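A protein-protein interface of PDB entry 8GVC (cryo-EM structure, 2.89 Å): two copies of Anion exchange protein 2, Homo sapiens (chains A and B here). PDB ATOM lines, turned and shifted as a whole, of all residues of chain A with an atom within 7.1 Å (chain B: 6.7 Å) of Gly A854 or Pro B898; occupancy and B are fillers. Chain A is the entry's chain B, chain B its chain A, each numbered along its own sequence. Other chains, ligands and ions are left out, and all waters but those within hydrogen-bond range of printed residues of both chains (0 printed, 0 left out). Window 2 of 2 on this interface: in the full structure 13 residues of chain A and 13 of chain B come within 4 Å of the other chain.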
ATOM      1  N   PRO A 851      28.575  -3.917 -26.042  1.00  0.00           N
ATOM      2  CA  PRO A 851      28.179  -4.493 -27.330  1.00  0.00           C
ATOM      3  C   PRO A 851      26.714  -4.901 -27.343  1.00  0.00           C
ATOM      4  O   PRO A 851      26.105  -5.187 -26.310  1.00  0.00           O
ATOM      5  CB  PRO A 851      29.097  -5.712 -27.474  1.00  0.00           C
ATOM      6  CG  PRO A 851      29.480  -6.058 -26.081  1.00  0.00           C
ATOM      7  CD  PRO A 851      29.536  -4.769 -25.324  1.00  0.00           C
ATOM      8  N   LEU A 852      26.148  -4.917 -28.547  1.00  0.00           N
ATOM      9  CA  LEU A 852      24.747  -5.282 -28.748  1.00  0.00           C
ATOM     10  C   LEU A 852      24.635  -6.800 -28.745  1.00  0.00           C
ATOM     11  O   LEU A 852      24.862  -7.454 -29.765  1.00  0.00           O
ATOM     12  CB  LEU A 852      24.221  -4.696 -30.052  1.00  0.00           C
ATOM     13  CG  LEU A 852      24.433  -3.203 -30.307  1.00  0.00           C
ATOM     14  CD1 LEU A 852      23.856  -2.817 -31.654  1.00  0.00           C
ATOM     15  CD2 LEU A 852      23.812  -2.372 -29.201  1.00  0.00           C
ATOM     16  N   HIS A 853      24.280  -7.369 -27.593  1.00  0.00           N
ATOM     17  CA  HIS A 853      24.128  -8.814 -27.459  1.00  0.00           C
ATOM     18  C   HIS A 853      22.686  -9.208 -27.174  1.00  0.00           C
ATOM     19  O   HIS A 853      22.123 -10.032 -27.902  1.00  0.00           O
ATOM     20  CB  HIS A 853      25.059  -9.337 -26.357  1.00  0.00           C
ATOM     21  CG  HIS A 853      26.475  -9.520 -26.803  1.00  0.00           C
ATOM     22  ND1 HIS A 853      27.549  -9.042 -26.083  1.00  0.00           N
ATOM     23  CD2 HIS A 853      26.995 -10.123 -27.898  1.00  0.00           C
ATOM     24  CE1 HIS A 853      28.669  -9.347 -26.713  1.00  0.00           C
ATOM     25  NE2 HIS A 853      28.362 -10.002 -27.818  1.00  0.00           N
ATOM     26  N   GLY A 854      22.071  -8.650 -26.136  1.00  0.00           N
ATOM     27  CA  GLY A 854      20.691  -8.959 -25.820  1.00  0.00           C
ATOM     28  C   GLY A 854      20.525 -10.250 -25.048  1.00  0.00           C
ATOM     29  O   GLY A 854      21.166 -11.257 -25.361  1.00  0.00           O
ATOM     30  N   CYS A 855      19.663 -10.233 -24.036  1.00  0.00           N
ATOM     31  CA  CYS A 855      19.399 -11.422 -23.234  1.00  0.00           C
ATOM     32  C   CYS A 855      18.117 -11.260 -22.423  1.00  0.00           C
ATOM     33  O   CYS A 855      17.610 -10.151 -22.261  1.00  0.00           O
ATOM     34  CB  CYS A 855      20.578 -11.716 -22.303  1.00  0.00           C
ATOM     35  SG  CYS A 855      20.417 -13.249 -21.359  1.00  0.00           S
ATOM     36  N   GLY A 896      28.560  -3.966 -20.249  1.00  0.00           N
ATOM     37  CA  GLY A 896      27.699  -4.918 -20.922  1.00  0.00           C
ATOM     38  C   GLY A 896      26.223  -4.614 -20.818  1.00  0.00           C
ATOM     39  O   GLY A 896      25.403  -5.510 -21.035  1.00  0.00           O
ATOM     40  N   PRO A 898      22.442  -3.251 -21.739  1.00  0.00           N
ATOM     41  CA  PRO A 898      21.693  -3.113 -22.993  1.00  0.00           C
ATOM     42  C   PRO A 898      21.048  -1.743 -23.139  1.00  0.00           C
ATOM     43  O   PRO A 898      20.712  -1.099 -22.139  1.00  0.00           O
ATOM     44  CB  PRO A 898      20.639  -4.221 -22.888  1.00  0.00           C
ATOM     45  CG  PRO A 898      20.494  -4.493 -21.400  1.00  0.00           C
ATOM     46  CD  PRO A 898      21.601  -3.787 -20.658  1.00  0.00           C
ATOM     47  N   ASN A 899      20.867  -1.289 -24.380  1.00  0.00           N
ATOM     48  CA  ASN A 899      20.201  -0.030 -24.700  1.00  0.00           C
ATOM     49  C   ASN A 899      21.027   1.196 -24.330  1.00  0.00           C
ATOM     50  O   ASN A 899      20.469   2.279 -24.139  1.00  0.00           O
ATOM     51  CB  ASN A 899      18.827   0.060 -24.026  1.00  0.00           C
ATOM     52  CG  ASN A 899      17.863  -0.995 -24.520  1.00  0.00           C
ATOM     53  OD1 ASN A 899      17.642  -1.137 -25.720  1.00  0.00           O
ATOM     54  ND2 ASN A 899      17.275  -1.738 -23.592  1.00  0.00           N
ATOM     55  N   LEU A 902      23.222   2.621 -28.171  1.00  0.00           N
ATOM     56  CA  LEU A 902      22.336   3.266 -29.133  1.00  0.00           C
ATOM     57  C   LEU A 902      21.732   4.543 -28.563  1.00  0.00           C
ATOM     58  O   LEU A 902      21.537   5.522 -29.293  1.00  0.00           O
ATOM     59  CB  LEU A 902      21.235   2.298 -29.565  1.00  0.00           C
ATOM     60  CG  LEU A 902      21.659   1.175 -30.512  1.00  0.00           C
ATOM     61  CD1 LEU A 902      20.610   0.082 -30.548  1.00  0.00           C
ATOM     62  CD2 LEU A 902      21.919   1.714 -31.905  1.00  0.00           C
ATOM     63  N   HIS B 850       8.024  -2.890 -27.653  1.00  0.00           N
ATOM     64  CA  HIS B 850       9.393  -3.252 -27.278  1.00  0.00           C
ATOM     65  C   HIS B 850       9.955  -2.191 -26.342  1.00  0.00           C
ATOM     66  O   HIS B 850      10.921  -1.498 -26.671  1.00  0.00           O
ATOM     67  CB  HIS B 850      10.275  -3.403 -28.516  1.00  0.00           C
ATOM     68  CG  HIS B 850       9.961  -4.605 -29.350  1.00  0.00           C
ATOM     69  ND1 HIS B 850      10.300  -5.885 -28.970  1.00  0.00           N
ATOM     70  CD2 HIS B 850       9.351  -4.719 -30.553  1.00  0.00           C
ATOM     71  CE1 HIS B 850       9.908  -6.737 -29.901  1.00  0.00           C
ATOM     72  NE2 HIS B 850       9.328  -6.055 -30.871  1.00  0.00           N
ATOM     73  N   PRO B 851       9.377  -2.045 -25.154  1.00  0.00           N
ATOM     74  CA  PRO B 851       9.801  -0.968 -24.255  1.00  0.00           C
ATOM     75  C   PRO B 851      11.228  -1.165 -23.767  1.00  0.00           C
ATOM     76  O   PRO B 851      11.753  -2.277 -23.711  1.00  0.00           O
ATOM     77  CB  PRO B 851       8.801  -1.055 -23.098  1.00  0.00           C
ATOM     78  CG  PRO B 851       8.309  -2.457 -23.129  1.00  0.00           C
ATOM     79  CD  PRO B 851       8.312  -2.873 -24.566  1.00  0.00           C
ATOM     80  N   LEU B 852      11.858  -0.047 -23.416  1.00  0.00           N
ATOM     81  CA  LEU B 852      13.234  -0.047 -22.924  1.00  0.00           C
ATOM     82  C   LEU B 852      13.221  -0.428 -21.450  1.00  0.00           C
ATOM     83  O   LEU B 852      12.967   0.409 -20.582  1.00  0.00           O
ATOM     84  CB  LEU B 852      13.881   1.318 -23.131  1.00  0.00           C
ATOM     85  CG  LEU B 852      13.802   1.944 -24.523  1.00  0.00           C
ATOM     86  CD1 LEU B 852      14.492   3.294 -24.526  1.00  0.00           C
ATOM     87  CD2 LEU B 852      14.414   1.028 -25.565  1.00  0.00           C
ATOM     88  N   GLY B 854      15.508  -3.578 -20.151  1.00  0.00           N
ATOM     89  CA  GLY B 854      16.834  -4.070 -19.838  1.00  0.00           C
ATOM     90  C   GLY B 854      16.840  -5.165 -18.792  1.00  0.00           C
ATOM     91  O   GLY B 854      16.126  -5.078 -17.788  1.00  0.00           O
ATOM     92  N   CYS B 855      17.642  -6.200 -19.015  1.00  0.00           N
ATOM     93  CA  CYS B 855      17.756  -7.301 -18.065  1.00  0.00           C
ATOM     94  C   CYS B 855      18.984  -8.155 -18.364  1.00  0.00           C
ATOM     95  O   CYS B 855      19.573  -8.059 -19.441  1.00  0.00           O
ATOM     96  CB  CYS B 855      16.494  -8.166 -18.091  1.00  0.00           C
ATOM     97  SG  CYS B 855      16.467  -9.480 -16.850  1.00  0.00           S
ATOM     98  N   GLY B 896       8.927  -7.656 -26.362  1.00  0.00           N
ATOM     99  CA  GLY B 896       9.788  -7.293 -25.246  1.00  0.00           C
ATOM    100  C   GLY B 896      11.256  -7.567 -25.487  1.00  0.00           C
ATOM    101  O   GLY B 896      11.946  -8.070 -24.592  1.00  0.00           O
ATOM    102  N   GLN B 897      11.756  -7.242 -26.682  1.00  0.00           N
ATOM    103  CA  GLN B 897      13.151  -7.486 -27.010  1.00  0.00           C
ATOM    104  C   GLN B 897      14.005  -6.259 -26.705  1.00  0.00           C
ATOM    105  O   GLN B 897      13.507  -5.129 -26.712  1.00  0.00           O
ATOM    106  CB  GLN B 897      13.294  -7.847 -28.485  1.00  0.00           C
ATOM    107  CG  GLN B 897      12.490  -9.060 -28.906  1.00  0.00           C
ATOM    108  CD  GLN B 897      13.090 -10.358 -28.410  1.00  0.00           C
ATOM    109  OE1 GLN B 897      12.581 -10.974 -27.476  1.00  0.00           O
ATOM    110  NE2 GLN B 897      14.178 -10.783 -29.040  1.00  0.00           N
ATOM    111  N   PRO B 898      15.289  -6.459 -26.421  1.00  0.00           N
ATOM    112  CA  PRO B 898      16.193  -5.329 -26.203  1.00  0.00           C
ATOM    113  C   PRO B 898      16.917  -4.909 -27.472  1.00  0.00           C
ATOM    114  O   PRO B 898      17.214  -5.715 -28.355  1.00  0.00           O
ATOM    115  CB  PRO B 898      17.183  -5.880 -25.167  1.00  0.00           C
ATOM    116  CG  PRO B 898      17.132  -7.385 -25.327  1.00  0.00           C
ATOM    117  CD  PRO B 898      15.964  -7.748 -26.205  1.00  0.00           C
ATOM    118  N   ASN B 899      17.203  -3.609 -27.547  1.00  0.00           N
ATOM    119  CA  ASN B 899      17.936  -3.002 -28.655  1.00  0.00           C
ATOM    120  C   ASN B 899      17.146  -2.996 -29.958  1.00  0.00           C
ATOM    121  O   ASN B 899      17.729  -2.805 -31.029  1.00  0.00           O
ATOM    122  CB  ASN B 899      19.282  -3.699 -28.878  1.00  0.00           C
ATOM    123  CG  ASN B 899      20.201  -3.588 -27.683  1.00  0.00           C
ATOM    124  OD1 ASN B 899      20.476  -2.495 -27.197  1.00  0.00           O
ATOM    125  ND2 ASN B 899      20.688  -4.725 -27.207  1.00  0.00           N
ATOM    126  N   THR B 900      15.832  -3.198 -29.901  1.00  0.00           N
ATOM    127  CA  THR B 900      15.006  -3.258 -31.103  1.00  0.00           C
ATOM    128  C   THR B 900      14.306  -1.944 -31.417  1.00  0.00           C
ATOM    129  O   THR B 900      14.169  -1.590 -32.590  1.00  0.00           O
ATOM    130  CB  THR B 900      13.958  -4.368 -30.972  1.00  0.00           C
ATOM    131  OG1 THR B 900      14.591  -5.644 -31.115  1.00  0.00           O
ATOM    132  CG2 THR B 900      12.899  -4.224 -32.044  1.00  0.00           C
ATOM    133  N   ALA B 901      13.861  -1.208 -30.398  1.00  0.00           N
ATOM    134  CA  ALA B 901      13.148   0.041 -30.637  1.00  0.00           C
ATOM    135  C   ALA B 901      14.077   1.172 -31.057  1.00  0.00           C
ATOM    136  O   ALA B 901      13.643   2.091 -31.759  1.00  0.00           O
ATOM    137  CB  ALA B 901      12.363   0.444 -29.391  1.00  0.00           C
ATOM    138  N   ASP B 956      22.756 -10.298 -33.913  1.00  0.00           N
ATOM    139  CA  ASP B 956      21.824 -10.887 -32.960  1.00  0.00           C
ATOM    140  C   ASP B 956      20.633  -9.992 -32.578  1.00  0.00           C
ATOM    141  O   ASP B 956      19.737 -10.423 -31.846  1.00  0.00           O
ATOM    142  CB  ASP B 956      22.532 -11.215 -31.644  1.00  0.00           C
ATOM    143  CG  ASP B 956      21.622 -11.911 -30.652  1.00  0.00           C
ATOM    144  OD1 ASP B 956      20.446 -12.158 -30.993  1.00  0.00           O
ATOM    145  OD2 ASP B 956      22.080 -12.215 -29.531  1.00  0.00           O
ATOM    146  N   THR B 957      20.607  -8.760 -33.075  1.00  0.00           N
ATOM    147  CA  THR B 957      19.491  -7.874 -32.779  1.00  0.00           C
ATOM    148  C   THR B 957      18.366  -8.305 -33.716  1.00  0.00           C
ATOM    149  O   THR B 957      18.599  -8.720 -34.854  1.00  0.00           O
ATOM    150  CB  THR B 957      19.793  -6.387 -32.968  1.00  0.00           C
ATOM    151  OG1 THR B 957      20.878  -6.010 -32.112  1.00  0.00           O
ATOM    152  CG2 THR B 957      18.578  -5.548 -32.621  1.00  0.00           C
ATOM    153  N   TYR B 958      17.134  -8.202 -33.226  1.00  0.00           N
ATOM    154  CA  TYR B 958      15.948  -8.605 -33.971  1.00  0.00           C
ATOM    155  C   TYR B 958      15.236  -7.375 -34.517  1.00  0.00           C
ATOM    156  O   TYR B 958      14.959  -6.431 -33.770  1.00  0.00           O
ATOM    157  CB  TYR B 958      14.991  -9.411 -33.091  1.00  0.00           C
ATOM    158  CG  TYR B 958      13.554  -9.346 -33.555  1.00  0.00           C
ATOM    159  CD1 TYR B 958      13.115 -10.115 -34.625  1.00  0.00           C
ATOM    160  CD2 TYR B 958      12.638  -8.511 -32.932  1.00  0.00           C
ATOM    161  CE1 TYR B 958      11.806 -10.056 -35.057  1.00  0.00           C
ATOM    162  CE2 TYR B 958      11.327  -8.445 -33.359  1.00  0.00           C
ATOM    163  CZ  TYR B 958      10.917  -9.219 -34.420  1.00  0.00           C
ATOM    164  OH  TYR B 958       9.612  -9.160 -34.849  1.00  0.00           O
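The side-chain amide oxygen (OD1) of Asn B899 lies within hydrogen-bond range of the backbone NH (N) of Asn A899 (3.1 Å). OD2 of Asp B956 lies close to O of His A853.
Leu A852 touches Asn B899 (CD2 to OD1, 3.9 Å). Gly A854 touches Pro B898 (CA to CG, 3.9 Å). Asn A899 touches Leu B852.
Gly A854 touches just one residue of chain B: Pro B898. Pro B898 touches just one residue of chain A: Gly A854 (3.9 Å). Of the printed residues of chain B, His A853 touches Asp B956. Of the printed residues of chain A, Asn B899 touches Leu A852 and Asn A899. Of the printed residues of chain A, Asp B956 touches His A853. Of the printed residues of chain B, Leu A852 touches Asn B899. Tyr B958 touches none of the printed residues of chain A. The nearest residue of chain B that does not touch Gly A854 is Asn B899 (4.3 Å).
Of the 9 printed residues of chain A, 4 touch a printed residue of chain B. Printed residues of chain A that touch a printed residue of chain B: Leu A852, His A853, Gly A854 and Asn A899. Hydrophobic or aromatic side chains of chain A that line the printed part of chain B: Leu A852. Along chain A the printed residues that touch a printed residue of chain B span positions 852 to 899. Hydrophobic or aromatic side chains of chain B within 4 Å of the printed part of chain A: Leu B852 and Pro B898.
Leu A852 touches Asn B899, and with the chains exchanged Asn A899 touches Leu B852. Gly A854 touches Pro B898, but with the chains exchanged Pro A898 does not touch Gly B854 (4.002 Å). Asn A899 touches its own counterpart, Asn B899. 7 positions are printed for both chains. Of the 5 pairs that touch across the chains among the printed residues, 3 have their exchanged pair printed and touching as well.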
